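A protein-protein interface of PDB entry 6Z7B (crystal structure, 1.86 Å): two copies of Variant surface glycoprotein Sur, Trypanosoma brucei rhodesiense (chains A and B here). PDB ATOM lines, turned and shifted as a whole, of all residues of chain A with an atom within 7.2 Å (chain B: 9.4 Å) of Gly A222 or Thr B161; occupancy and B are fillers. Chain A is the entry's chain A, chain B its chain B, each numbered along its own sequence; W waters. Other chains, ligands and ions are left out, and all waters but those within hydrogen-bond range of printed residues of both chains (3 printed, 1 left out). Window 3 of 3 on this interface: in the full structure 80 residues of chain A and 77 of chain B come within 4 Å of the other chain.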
ATOM      1  N   THR A 161       1.638 -35.587  27.109  1.00  0.00           N
ATOM      2  CA  THR A 161       0.936 -36.473  28.019  1.00  0.00           C
ATOM      3  C   THR A 161      -0.565 -36.490  27.751  1.00  0.00           C
ATOM      4  O   THR A 161      -1.259 -37.419  28.173  1.00  0.00           O
ATOM      5  CB  THR A 161       1.239 -36.080  29.472  1.00  0.00           C
ATOM      6  OG1 THR A 161       0.655 -34.809  29.783  1.00  0.00           O
ATOM      7  CG2 THR A 161       2.743 -35.990  29.679  1.00  0.00           C
ATOM      8  N   GLY A 219      -5.602 -24.785  24.220  1.00  0.00           N
ATOM      9  CA  GLY A 219      -5.691 -24.452  25.629  1.00  0.00           C
ATOM     10  C   GLY A 219      -5.589 -25.673  26.518  1.00  0.00           C
ATOM     11  O   GLY A 219      -6.171 -26.715  26.218  1.00  0.00           O
ATOM     12  N   SER A 220      -4.856 -25.562  27.619  1.00  0.00           N
ATOM     13  CA  SER A 220      -4.631 -26.691  28.504  1.00  0.00           C
ATOM     14  C   SER A 220      -4.967 -26.300  29.936  1.00  0.00           C
ATOM     15  O   SER A 220      -4.967 -25.125  30.305  1.00  0.00           O
ATOM     16  CB  SER A 220      -3.184 -27.193  28.423  1.00  0.00           C
ATOM     17  OG  SER A 220      -3.079 -28.503  28.946  1.00  0.00           O
ATOM     18  N   LYS A 221      -5.260 -27.313  30.739  1.00  0.00           N
ATOM     19  CA  LYS A 221      -5.548 -27.109  32.149  1.00  0.00           C
ATOM     20  C   LYS A 221      -5.265 -28.415  32.861  1.00  0.00           C
ATOM     21  O   LYS A 221      -5.645 -29.478  32.365  1.00  0.00           O
ATOM     22  CB  LYS A 221      -7.002 -26.682  32.354  1.00  0.00           C
ATOM     23  CG  LYS A 221      -7.399 -26.483  33.787  1.00  0.00           C
ATOM     24  CD  LYS A 221      -8.893 -26.342  33.905  1.00  0.00           C
ATOM     25  CE  LYS A 221      -9.246 -25.678  35.208  1.00  0.00           C
ATOM     26  NZ  LYS A 221     -10.553 -26.140  35.724  1.00  0.00           N
ATOM     27  N   GLY A 222      -4.587 -28.340  33.995  1.00  0.00           N
ATOM     28  CA  GLY A 222      -4.332 -29.546  34.764  1.00  0.00           C
ATOM     29  C   GLY A 222      -3.453 -30.526  34.010  1.00  0.00           C
ATOM     30  O   GLY A 222      -2.426 -30.168  33.415  1.00  0.00           O
ATOM     31  N   ASN A 223      -3.874 -31.788  34.027  1.00  0.00           N
ATOM     32  CA  ASN A 223      -3.131 -32.891  33.423  1.00  0.00           C
ATOM     33  C   ASN A 223      -4.046 -33.617  32.447  1.00  0.00           C
ATOM     34  O   ASN A 223      -4.559 -34.702  32.752  1.00  0.00           O
ATOM     35  CB  ASN A 223      -2.609 -33.850  34.491  1.00  0.00           C
ATOM     36  CG  ASN A 223      -1.300 -34.496  34.101  1.00  0.00           C
ATOM     37  OD1 ASN A 223      -0.260 -33.828  34.043  1.00  0.00           O
ATOM     38  ND2 ASN A 223      -1.336 -35.804  33.840  1.00  0.00           N
ATOM     39  N   PRO A 224      -4.287 -33.038  31.271  1.00  0.00           N
ATOM     40  CA  PRO A 224      -5.091 -33.739  30.265  1.00  0.00           C
ATOM     41  C   PRO A 224      -4.399 -35.016  29.812  1.00  0.00           C
ATOM     42  O   PRO A 224      -3.187 -35.043  29.571  1.00  0.00           O
ATOM     43  CB  PRO A 224      -5.209 -32.723  29.120  1.00  0.00           C
ATOM     44  CG  PRO A 224      -4.815 -31.411  29.710  1.00  0.00           C
ATOM     45  CD  PRO A 224      -3.843 -31.717  30.801  1.00  0.00           C
ATOM     46  N   ASP A 238     -11.230 -34.035  31.836  1.00  0.00           N
ATOM     47  CA  ASP A 238     -10.764 -35.251  32.488  1.00  0.00           C
ATOM     48  C   ASP A 238     -11.560 -35.589  33.719  1.00  0.00           C
ATOM     49  O   ASP A 238     -12.516 -36.366  33.656  1.00  0.00           O
ATOM     50  CB  ASP A 238      -9.295 -35.126  32.885  1.00  0.00           C
ATOM     51  CG  ASP A 238      -8.562 -36.446  32.857  1.00  0.00           C
ATOM     52  OD1 ASP A 238      -7.311 -36.441  32.760  1.00  0.00           O
ATOM     53  OD2 ASP A 238      -9.240 -37.490  32.936  1.00  0.00           O
ATOM     54  N   PHE A 246     -13.365 -24.586  30.942  1.00  0.00           N
ATOM     55  CA  PHE A 246     -12.516 -25.719  31.279  1.00  0.00           C
ATOM     56  C   PHE A 246     -12.903 -26.217  32.671  1.00  0.00           C
ATOM     57  O   PHE A 246     -12.149 -26.115  33.643  1.00  0.00           O
ATOM     58  CB  PHE A 246     -11.016 -25.319  31.171  1.00  0.00           C
ATOM     59  CG  PHE A 246     -10.411 -25.543  29.792  1.00  0.00           C
ATOM     60  CD1 PHE A 246     -11.199 -25.916  28.720  1.00  0.00           C
ATOM     61  CD2 PHE A 246      -9.047 -25.397  29.586  1.00  0.00           C
ATOM     62  CE1 PHE A 246     -10.638 -26.133  27.476  1.00  0.00           C
ATOM     63  CE2 PHE A 246      -8.481 -25.614  28.339  1.00  0.00           C
ATOM     64  CZ  PHE A 246      -9.272 -25.975  27.289  1.00  0.00           C
ATOM     65  N   GLY A 248     -13.495 -29.290  34.018  1.00  0.00           N
ATOM     66  CA  GLY A 248     -12.771 -30.384  34.630  1.00  0.00           C
ATOM     67  C   GLY A 248     -11.383 -29.973  35.078  1.00  0.00           C
ATOM     68  O   GLY A 248     -10.786 -29.021  34.583  1.00  0.00           O
ATOM     69  N   ALA A 249     -10.864 -30.707  36.058  1.00  0.00           N
ATOM     70  CA  ALA A 249      -9.534 -30.393  36.560  1.00  0.00           C
ATOM     71  C   ALA A 249      -8.490 -30.505  35.460  1.00  0.00           C
ATOM     72  O   ALA A 249      -7.483 -29.791  35.478  1.00  0.00           O
ATOM     73  CB  ALA A 249      -9.187 -31.302  37.743  1.00  0.00           C
ATOM     74  N   ASN A 250      -8.715 -31.373  34.481  1.00  0.00           N
ATOM     75  CA  ASN A 250      -7.791 -31.510  33.363  1.00  0.00           C
ATOM     76  C   ASN A 250      -8.557 -31.368  32.055  1.00  0.00           C
ATOM     77  O   ASN A 250      -9.397 -32.210  31.733  1.00  0.00           O
ATOM     78  CB  ASN A 250      -7.048 -32.835  33.429  1.00  0.00           C
ATOM     79  CG  ASN A 250      -6.665 -33.205  34.835  1.00  0.00           C
ATOM     80  OD1 ASN A 250      -5.717 -32.658  35.394  1.00  0.00           O
ATOM     81  ND2 ASN A 250      -7.411 -34.127  35.428  1.00  0.00           N
ATOM     82  N   ALA A 251      -8.261 -30.306  31.309  1.00  0.00           N
ATOM     83  CA  ALA A 251      -8.915 -30.015  30.045  1.00  0.00           C
ATOM     84  C   ALA A 251      -7.877 -29.703  28.971  1.00  0.00           C
ATOM     85  O   ALA A 251      -6.782 -29.205  29.257  1.00  0.00           O
ATOM     86  CB  ALA A 251      -9.892 -28.850  30.193  1.00  0.00           C
ATOM     87  N   ALA B 150       2.626 -17.884  23.570  1.00  0.00           N
ATOM     88  CA  ALA B 150       2.151 -18.561  24.771  1.00  0.00           C
ATOM     89  C   ALA B 150       1.345 -17.604  25.632  1.00  0.00           C
ATOM     90  O   ALA B 150       1.791 -16.489  25.905  1.00  0.00           O
ATOM     91  CB  ALA B 150       3.326 -19.117  25.565  1.00  0.00           C
ATOM     92  N   GLY B 151       0.155 -18.038  26.059  1.00  0.00           N
ATOM     93  CA  GLY B 151      -0.691 -17.243  26.925  1.00  0.00           C
ATOM     94  C   GLY B 151      -1.211 -18.046  28.105  1.00  0.00           C
ATOM     95  O   GLY B 151      -0.891 -19.224  28.282  1.00  0.00           O
ATOM     96  N   GLY B 152      -2.012 -17.370  28.911  1.00  0.00           N
ATOM     97  CA  GLY B 152      -2.734 -18.034  29.967  1.00  0.00           C
ATOM     98  C   GLY B 152      -4.170 -18.184  29.541  1.00  0.00           C
ATOM     99  O   GLY B 152      -4.422 -18.624  28.428  1.00  0.00           O
ATOM    100  N   ALA B 153      -5.119 -17.815  30.390  1.00  0.00           N
ATOM    101  CA  ALA B 153      -6.519 -17.837  29.996  1.00  0.00           C
ATOM    102  C   ALA B 153      -6.800 -16.652  29.088  1.00  0.00           C
ATOM    103  O   ALA B 153      -6.580 -15.501  29.472  1.00  0.00           O
ATOM    104  CB  ALA B 153      -7.430 -17.798  31.217  1.00  0.00           C
ATOM    105  N   GLN B 154      -7.256 -16.944  27.873  1.00  0.00           N
ATOM    106  CA  GLN B 154      -7.717 -15.946  26.923  1.00  0.00           C
ATOM    107  C   GLN B 154      -8.800 -16.590  26.075  1.00  0.00           C
ATOM    108  O   GLN B 154      -8.825 -17.811  25.916  1.00  0.00           O
ATOM    109  CB  GLN B 154      -6.581 -15.436  26.032  1.00  0.00           C
ATOM    110  CG  GLN B 154      -5.912 -16.524  25.222  1.00  0.00           C
ATOM    111  CD  GLN B 154      -4.751 -16.004  24.420  1.00  0.00           C
ATOM    112  OE1 GLN B 154      -4.867 -14.996  23.731  1.00  0.00           O
ATOM    113  NE2 GLN B 154      -3.616 -16.681  24.512  1.00  0.00           N
ATOM    114  N   PHE B 157     -10.712 -19.689  25.551  1.00  0.00           N
ATOM    115  CA  PHE B 157     -10.343 -20.645  26.596  1.00  0.00           C
ATOM    116  C   PHE B 157     -10.130 -19.882  27.908  1.00  0.00           C
ATOM    117  O   PHE B 157      -8.999 -19.673  28.363  1.00  0.00           O
ATOM    118  CB  PHE B 157      -9.113 -21.438  26.176  1.00  0.00           C
ATOM    119  CG  PHE B 157      -9.367 -22.396  25.043  1.00  0.00           C
ATOM    120  CD1 PHE B 157     -10.514 -23.178  25.019  1.00  0.00           C
ATOM    121  CD2 PHE B 157      -8.460 -22.522  24.009  1.00  0.00           C
ATOM    122  CE1 PHE B 157     -10.750 -24.067  23.983  1.00  0.00           C
ATOM    123  CE2 PHE B 157      -8.693 -23.406  22.978  1.00  0.00           C
ATOM    124  CZ  PHE B 157      -9.839 -24.181  22.968  1.00  0.00           C
ATOM    125  N   SER B 158     -11.238 -19.475  28.527  1.00  0.00           N
ATOM    126  CA  SER B 158     -11.187 -18.696  29.755  1.00  0.00           C
ATOM    127  C   SER B 158     -10.901 -19.540  30.986  1.00  0.00           C
ATOM    128  O   SER B 158     -10.813 -18.984  32.085  1.00  0.00           O
ATOM    129  CB  SER B 158     -12.495 -17.932  29.949  1.00  0.00           C
ATOM    130  OG  SER B 158     -13.583 -18.818  30.104  1.00  0.00           O
ATOM    131  N   GLY B 159     -10.754 -20.852  30.843  1.00  0.00           N
ATOM    132  CA  GLY B 159     -10.421 -21.680  31.980  1.00  0.00           C
ATOM    133  C   GLY B 159      -9.043 -22.297  31.890  1.00  0.00           C
ATOM    134  O   GLY B 159      -8.645 -23.061  32.770  1.00  0.00           O
ATOM    135  N   ALA B 160      -8.299 -21.977  30.839  1.00  0.00           N
ATOM    136  CA  ALA B 160      -7.023 -22.635  30.616  1.00  0.00           C
ATOM    137  C   ALA B 160      -5.957 -22.086  31.556  1.00  0.00           C
ATOM    138  O   ALA B 160      -6.005 -20.934  31.977  1.00  0.00           O
ATOM    139  CB  ALA B 160      -6.587 -22.473  29.157  1.00  0.00           C
ATOM    140  N   THR B 161      -5.004 -22.941  31.907  1.00  0.00           N
ATOM    141  CA  THR B 161      -3.775 -22.509  32.558  1.00  0.00           C
ATOM    142  C   THR B 161      -2.713 -22.102  31.549  1.00  0.00           C
ATOM    143  O   THR B 161      -1.869 -21.245  31.836  1.00  0.00           O
ATOM    144  CB  THR B 161      -3.231 -23.634  33.435  1.00  0.00           C
ATOM    145  OG1 THR B 161      -2.442 -24.547  32.642  1.00  0.00           O
ATOM    146  CG2 THR B 161      -4.393 -24.373  34.050  1.00  0.00           C
ATOM    147  N   GLY B 162      -2.742 -22.707  30.374  1.00  0.00           N
ATOM    148  CA  GLY B 162      -1.907 -22.258  29.291  1.00  0.00           C
ATOM    149  C   GLY B 162      -2.666 -22.279  27.990  1.00  0.00           C
ATOM    150  O   GLY B 162      -3.535 -23.132  27.779  1.00  0.00           O
ATOM    151  N   THR B 163      -2.368 -21.311  27.130  1.00  0.00           N
ATOM    152  CA  THR B 163      -2.851 -21.290  25.767  1.00  0.00           C
ATOM    153  C   THR B 163      -1.661 -21.042  24.860  1.00  0.00           C
ATOM    154  O   THR B 163      -0.683 -20.400  25.251  1.00  0.00           O
ATOM    155  CB  THR B 163      -3.927 -20.224  25.540  1.00  0.00           C
ATOM    156  OG1 THR B 163      -3.511 -18.997  26.147  1.00  0.00           O
ATOM    157  CG2 THR B 163      -5.278 -20.658  26.119  1.00  0.00           C
ATOM    158  N   CYS B 164      -1.755 -21.580  23.648  1.00  0.00           N
ATOM    159  CA  CYS B 164      -0.726 -21.476  22.621  1.00  0.00           C
ATOM    160  C   CYS B 164      -1.419 -21.033  21.347  1.00  0.00           C
ATOM    161  O   CYS B 164      -2.113 -21.836  20.715  1.00  0.00           O
ATOM    162  CB  CYS B 164      -0.031 -22.812  22.421  1.00  0.00           C
ATOM    163  SG  CYS B 164       1.590 -22.681  21.642  1.00  0.00           S
ATOM    164  N   SER B 220      -0.458 -31.451  24.905  1.00  0.00           N
ATOM    165  CA  SER B 220      -0.068 -30.759  26.121  1.00  0.00           C
ATOM    166  C   SER B 220       0.819 -31.666  26.961  1.00  0.00           C
ATOM    167  O   SER B 220       0.776 -32.894  26.854  1.00  0.00           O
ATOM    168  CB  SER B 220      -1.290 -30.305  26.930  1.00  0.00           C
ATOM    169  OG  SER B 220      -0.903 -29.739  28.164  1.00  0.00           O
ATOM    170  N   LYS B 221       1.634 -31.036  27.795  1.00  0.00           N
ATOM    171  CA  LYS B 221       2.579 -31.750  28.637  1.00  0.00           C
ATOM    172  C   LYS B 221       2.888 -30.896  29.851  1.00  0.00           C
ATOM    173  O   LYS B 221       3.269 -29.736  29.713  1.00  0.00           O
ATOM    174  CB  LYS B 221       3.866 -32.073  27.879  1.00  0.00           C
ATOM    175  CG  LYS B 221       4.979 -32.559  28.772  1.00  0.00           C
ATOM    176  CD  LYS B 221       6.305 -32.577  28.049  1.00  0.00           C
ATOM    177  CE  LYS B 221       7.309 -33.365  28.881  1.00  0.00           C
ATOM    178  NZ  LYS B 221       8.658 -33.450  28.284  1.00  0.00           N
ATOM    179  N   GLY B 222       2.725 -31.461  31.032  1.00  0.00           N
ATOM    180  CA  GLY B 222       3.090 -30.706  32.217  1.00  0.00           C
ATOM    181  C   GLY B 222       2.128 -29.562  32.451  1.00  0.00           C
ATOM    182  O   GLY B 222       0.903 -29.720  32.377  1.00  0.00           O
ATOM    183  N   ASN B 223       2.689 -28.384  32.731  1.00  0.00           N
ATOM    184  CA  ASN B 223       1.924 -27.206  33.131  1.00  0.00           C
ATOM    185  C   ASN B 223       2.240 -26.063  32.173  1.00  0.00           C
ATOM    186  O   ASN B 223       3.055 -25.183  32.492  1.00  0.00           O
ATOM    187  CB  ASN B 223       2.239 -26.834  34.580  1.00  0.00           C
ATOM    188  CG  ASN B 223       1.415 -25.674  35.081  1.00  0.00           C
ATOM    189  OD1 ASN B 223       0.279 -25.479  34.658  1.00  0.00           O
ATOM    190  ND2 ASN B 223       1.985 -24.889  35.984  1.00  0.00           N
ATOM    191  N   PRO B 224       1.616 -26.040  30.990  1.00  0.00           N
ATOM    192  CA  PRO B 224       1.836 -24.928  30.053  1.00  0.00           C
ATOM    193  C   PRO B 224       1.210 -23.644  30.578  1.00  0.00           C
ATOM    194  O   PRO B 224       0.067 -23.638  31.038  1.00  0.00           O
ATOM    195  CB  PRO B 224       1.148 -25.397  28.762  1.00  0.00           C
ATOM    196  CG  PRO B 224       0.655 -26.783  29.013  1.00  0.00           C
ATOM    197  CD  PRO B 224       0.606 -26.985  30.493  1.00  0.00           C
ATOM    198  N   THR B 225       1.979 -22.560  30.533  1.00  0.00           N
ATOM    199  CA  THR B 225       1.521 -21.266  31.025  1.00  0.00           C
ATOM    200  C   THR B 225       1.986 -20.190  30.060  1.00  0.00           C
ATOM    201  O   THR B 225       2.595 -20.475  29.027  1.00  0.00           O
ATOM    202  CB  THR B 225       2.027 -20.965  32.450  1.00  0.00           C
ATOM    203  OG1 THR B 225       3.319 -20.363  32.391  1.00  0.00           O
ATOM    204  CG2 THR B 225       2.128 -22.223  33.292  1.00  0.00           C
ATOM    205  N   GLN B 226       1.705 -18.932  30.406  1.00  0.00           N
ATOM    206  CA  GLN B 226       2.186 -17.828  29.587  1.00  0.00           C
ATOM    207  C   GLN B 226       3.706 -17.721  29.615  1.00  0.00           C
ATOM    208  O   GLN B 226       4.293 -17.108  28.719  1.00  0.00           O
ATOM    209  CB  GLN B 226       1.543 -16.514  30.031  1.00  0.00           C
ATOM    210  CG  GLN B 226       1.880 -15.325  29.147  1.00  0.00           C
ATOM    211  CD  GLN B 226       1.410 -13.995  29.713  1.00  0.00           C
ATOM    212  OE1 GLN B 226       0.242 -13.829  30.069  1.00  0.00           O
ATOM    213  NE2 GLN B 226       2.328 -13.036  29.797  1.00  0.00           N
ATOM    214  N   SER B 227       4.361 -18.332  30.601  1.00  0.00           N
ATOM    215  CA  SER B 227       5.814 -18.387  30.590  1.00  0.00           C
ATOM    216  C   SER B 227       6.356 -19.422  29.618  1.00  0.00           C
ATOM    217  O   SER B 227       7.580 -19.519  29.467  1.00  0.00           O
ATOM    218  CB  SER B 227       6.341 -18.682  31.986  1.00  0.00           C
ATOM    219  OG  SER B 227       6.345 -20.080  32.203  1.00  0.00           O
ATOM    220  N   SER B 228       5.486 -20.178  28.944  1.00  0.00           N
ATOM    221  CA  SER B 228       5.931 -21.207  28.017  1.00  0.00           C
ATOM    222  C   SER B 228       6.345 -20.574  26.694  1.00  0.00           C
ATOM    223  O   SER B 228       5.863 -20.965  25.630  1.00  0.00           O
ATOM    224  CB  SER B 228       4.828 -22.252  27.826  1.00  0.00           C
ATOM    225  OG  SER B 228       4.623 -22.993  29.023  1.00  0.00           O
ATOM    226  N   ASP B 238       8.395 -24.341  28.169  1.00  0.00           N
ATOM    227  CA  ASP B 238       9.279 -23.709  29.141  1.00  0.00           C
ATOM    228  C   ASP B 238       9.699 -24.754  30.158  1.00  0.00           C
ATOM    229  O   ASP B 238       8.998 -25.749  30.365  1.00  0.00           O
ATOM    230  CB  ASP B 238       8.631 -22.507  29.852  1.00  0.00           C
ATOM    231  CG  ASP B 238       7.467 -22.896  30.770  1.00  0.00           C
ATOM    232  OD1 ASP B 238       6.811 -23.918  30.547  1.00  0.00           O
ATOM    233  OD2 ASP B 238       7.184 -22.149  31.717  1.00  0.00           O
ATOM    234  N   ASN B 250       7.207 -28.212  30.450  1.00  0.00           N
ATOM    235  CA  ASN B 250       5.829 -27.883  30.126  1.00  0.00           C
ATOM    236  C   ASN B 250       5.761 -27.515  28.653  1.00  0.00           C
ATOM    237  O   ASN B 250       6.681 -26.886  28.125  1.00  0.00           O
ATOM    238  CB  ASN B 250       5.318 -26.716  30.967  1.00  0.00           C
ATOM    239  CG  ASN B 250       5.744 -26.812  32.408  1.00  0.00           C
ATOM    240  OD1 ASN B 250       5.250 -27.651  33.155  1.00  0.00           O
ATOM    241  ND2 ASN B 250       6.670 -25.949  32.810  1.00  0.00           N
ATOM    242  N   ALA B 251       4.671 -27.902  27.998  1.00  0.00           N
ATOM    243  CA  ALA B 251       4.542 -27.696  26.567  1.00  0.00           C
ATOM    244  C   ALA B 251       3.069 -27.666  26.201  1.00  0.00           C
ATOM    245  O   ALA B 251       2.251 -28.328  26.833  1.00  0.00           O
ATOM    246  CB  ALA B 251       5.266 -28.786  25.788  1.00  0.00           C
ATOM    247  N   LEU B 252       2.743 -26.866  25.188  1.00  0.00           N
ATOM    248  CA  LEU B 252       1.423 -26.873  24.571  1.00  0.00           C
ATOM    249  C   LEU B 252       1.602 -26.527  23.101  1.00  0.00           C
ATOM    250  O   LEU B 252       2.546 -25.829  22.725  1.00  0.00           O
ATOM    251  CB  LEU B 252       0.445 -25.891  25.248  1.00  0.00           C
ATOM    252  CG  LEU B 252      -1.006 -25.810  24.740  1.00  0.00           C
ATOM    253  CD1 LEU B 252      -1.757 -27.107  24.899  1.00  0.00           C
ATOM    254  CD2 LEU B 252      -1.751 -24.696  25.425  1.00  0.00           C
HETATM  255  O   HOH W   1      -0.532 -31.021  30.622  1.00  0.00           O
HETATM  256  O   HOH W   2       2.353 -33.804  32.081  1.00  0.00           O
HETATM  257  O   HOH W   3      -2.252 -27.428  31.849  1.00  0.00           O
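Among the printed residues, pairs that only touch across the chains: Thr A161 with Lys B221, Gly A219 with Phe B157, Gly A219 with Gly B162, Gly A219 with Thr B163, Gly A219 with Leu B252, Ser A220 with Ala B160, Ser A220 with Pro B224, Ser A220 with Leu B252, Lys A221 with Gly B159, Lys A221 with Thr B161, Gly A222 with Thr B161, Gly A222 with Gly B222, Phe A246 with Phe B157, Phe A246 with Gly B159 and Phe A246 with Ala B160.
Hydrophobic or aromatic side chains of chain A that line the printed part of chain B: Phe A246.
Among the printed residues, 19 pairs touch across the chains.
Among the printed residues, no Asp or Glu carboxylate lies within 4 Å of a Lys or Arg side-chain nitrogen of the other chain.
The side-chain hydroxyl of Ser A220 is in hydrogen-bond range of the side-chain hydroxyl of Ser B220 (2.6 Å).
The backbone NH of Thr A161 is in hydrogen-bond range of the backbone carbonyl oxygen of Ser B220, at 2.8 Å.
The backbone carbonyl oxygen (O) of Gly B162 lies within hydrogen-bond range of the backbone NH (N) of Ser A220.
The backbone carbonyl oxygen (O) of Ser A220 sits at hydrogen-bond distance from the backbone NH (N) of Thr B161 (2.7 Å).
Water W2 lies within hydrogen-bond range of the backbone NH of Gly B222 (2.6 Å), the side-chain hydroxyl of Thr A161 (3.0 Å) and the side-chain amide oxygen of Asn A223 (3.3 Å).
Water W1 lies within hydrogen-bond range of the backbone carbonyl oxygen of Gly B222, the side-chain hydroxyl of Ser B220 and the backbone carbonyl oxygen of Gly A222.
Water W3 lies within hydrogen-bond range of the side-chain hydroxyl of Thr B161 (3.0 Å), the backbone carbonyl oxygen of Gly A222 (3.2 Å), the side-chain hydroxyl of Ser A220 (3.2 Å) and the backbone NH of Lys A221 (3.2 Å).
Thr A161 touches Lys B221, and with the chains exchanged Lys A221 touches Thr B161.
Ser A220 touches its own counterpart, Ser B220.
Gly A222 touches Thr B161, but with the chains exchanged Thr A161 does not touch Gly B222 (4.1 Å).
Gly B222 touches its own counterpart, Gly A222.
Gly A222 touches just these residues of chain B: Thr B161 (3.97 Å) and Gly B222 (3.5 Å).
Of chain A, only Ser A220 (2.7 Å), Lys A221 (3.5 Å) and Gly A222 (3.97 Å) come within 4 Å of Thr B161.
Of chain B, only Ala B160, Thr B161, Gly B162, Ser B220, Pro B224 and Leu B252 come within 4 Å of Ser A220.
Of the printed residues of chain B, Thr A161 touches Ser B220 (2.8 Å) and Lys B221 (3.8 Å).
Printed residues of chain B within 4 Å of Gly A219: Phe B157 (3.6 Å), Gly B162 (3.3 Å), Thr B163 (3.8 Å) and Leu B252 (3.95 Å).
Ser B228 touches none of the printed residues of chain A.
The nearest printed residue of chain A that does not touch Lys B221 is Ser A220 (5.5 Å).
The backbone carbonyl oxygen of Lys B221 lies within hydrogen-bond range of the backbone NH of Ala B251, 2.9 Å away.
The side-chain amide nitrogen of Gln B154 is in hydrogen-bond range of the side-chain hydroxyl of Thr B163 (2.8 Å).
O of Pro B224 sits close to N of Gly B162, 3.0 Å away.
The backbone carbonyl oxygen of Gly A248 is in hydrogen-bond range of the side-chain amino group of Lys A221, 3.1 Å away.
The backbone carbonyl oxygen of Phe A246 lies within hydrogen-bond range of the side-chain amino group of Lys A221 (2.6 Å).
N of Gly B151 lies within hydrogen-bond range of O of Thr B163, at 2.6 Å.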
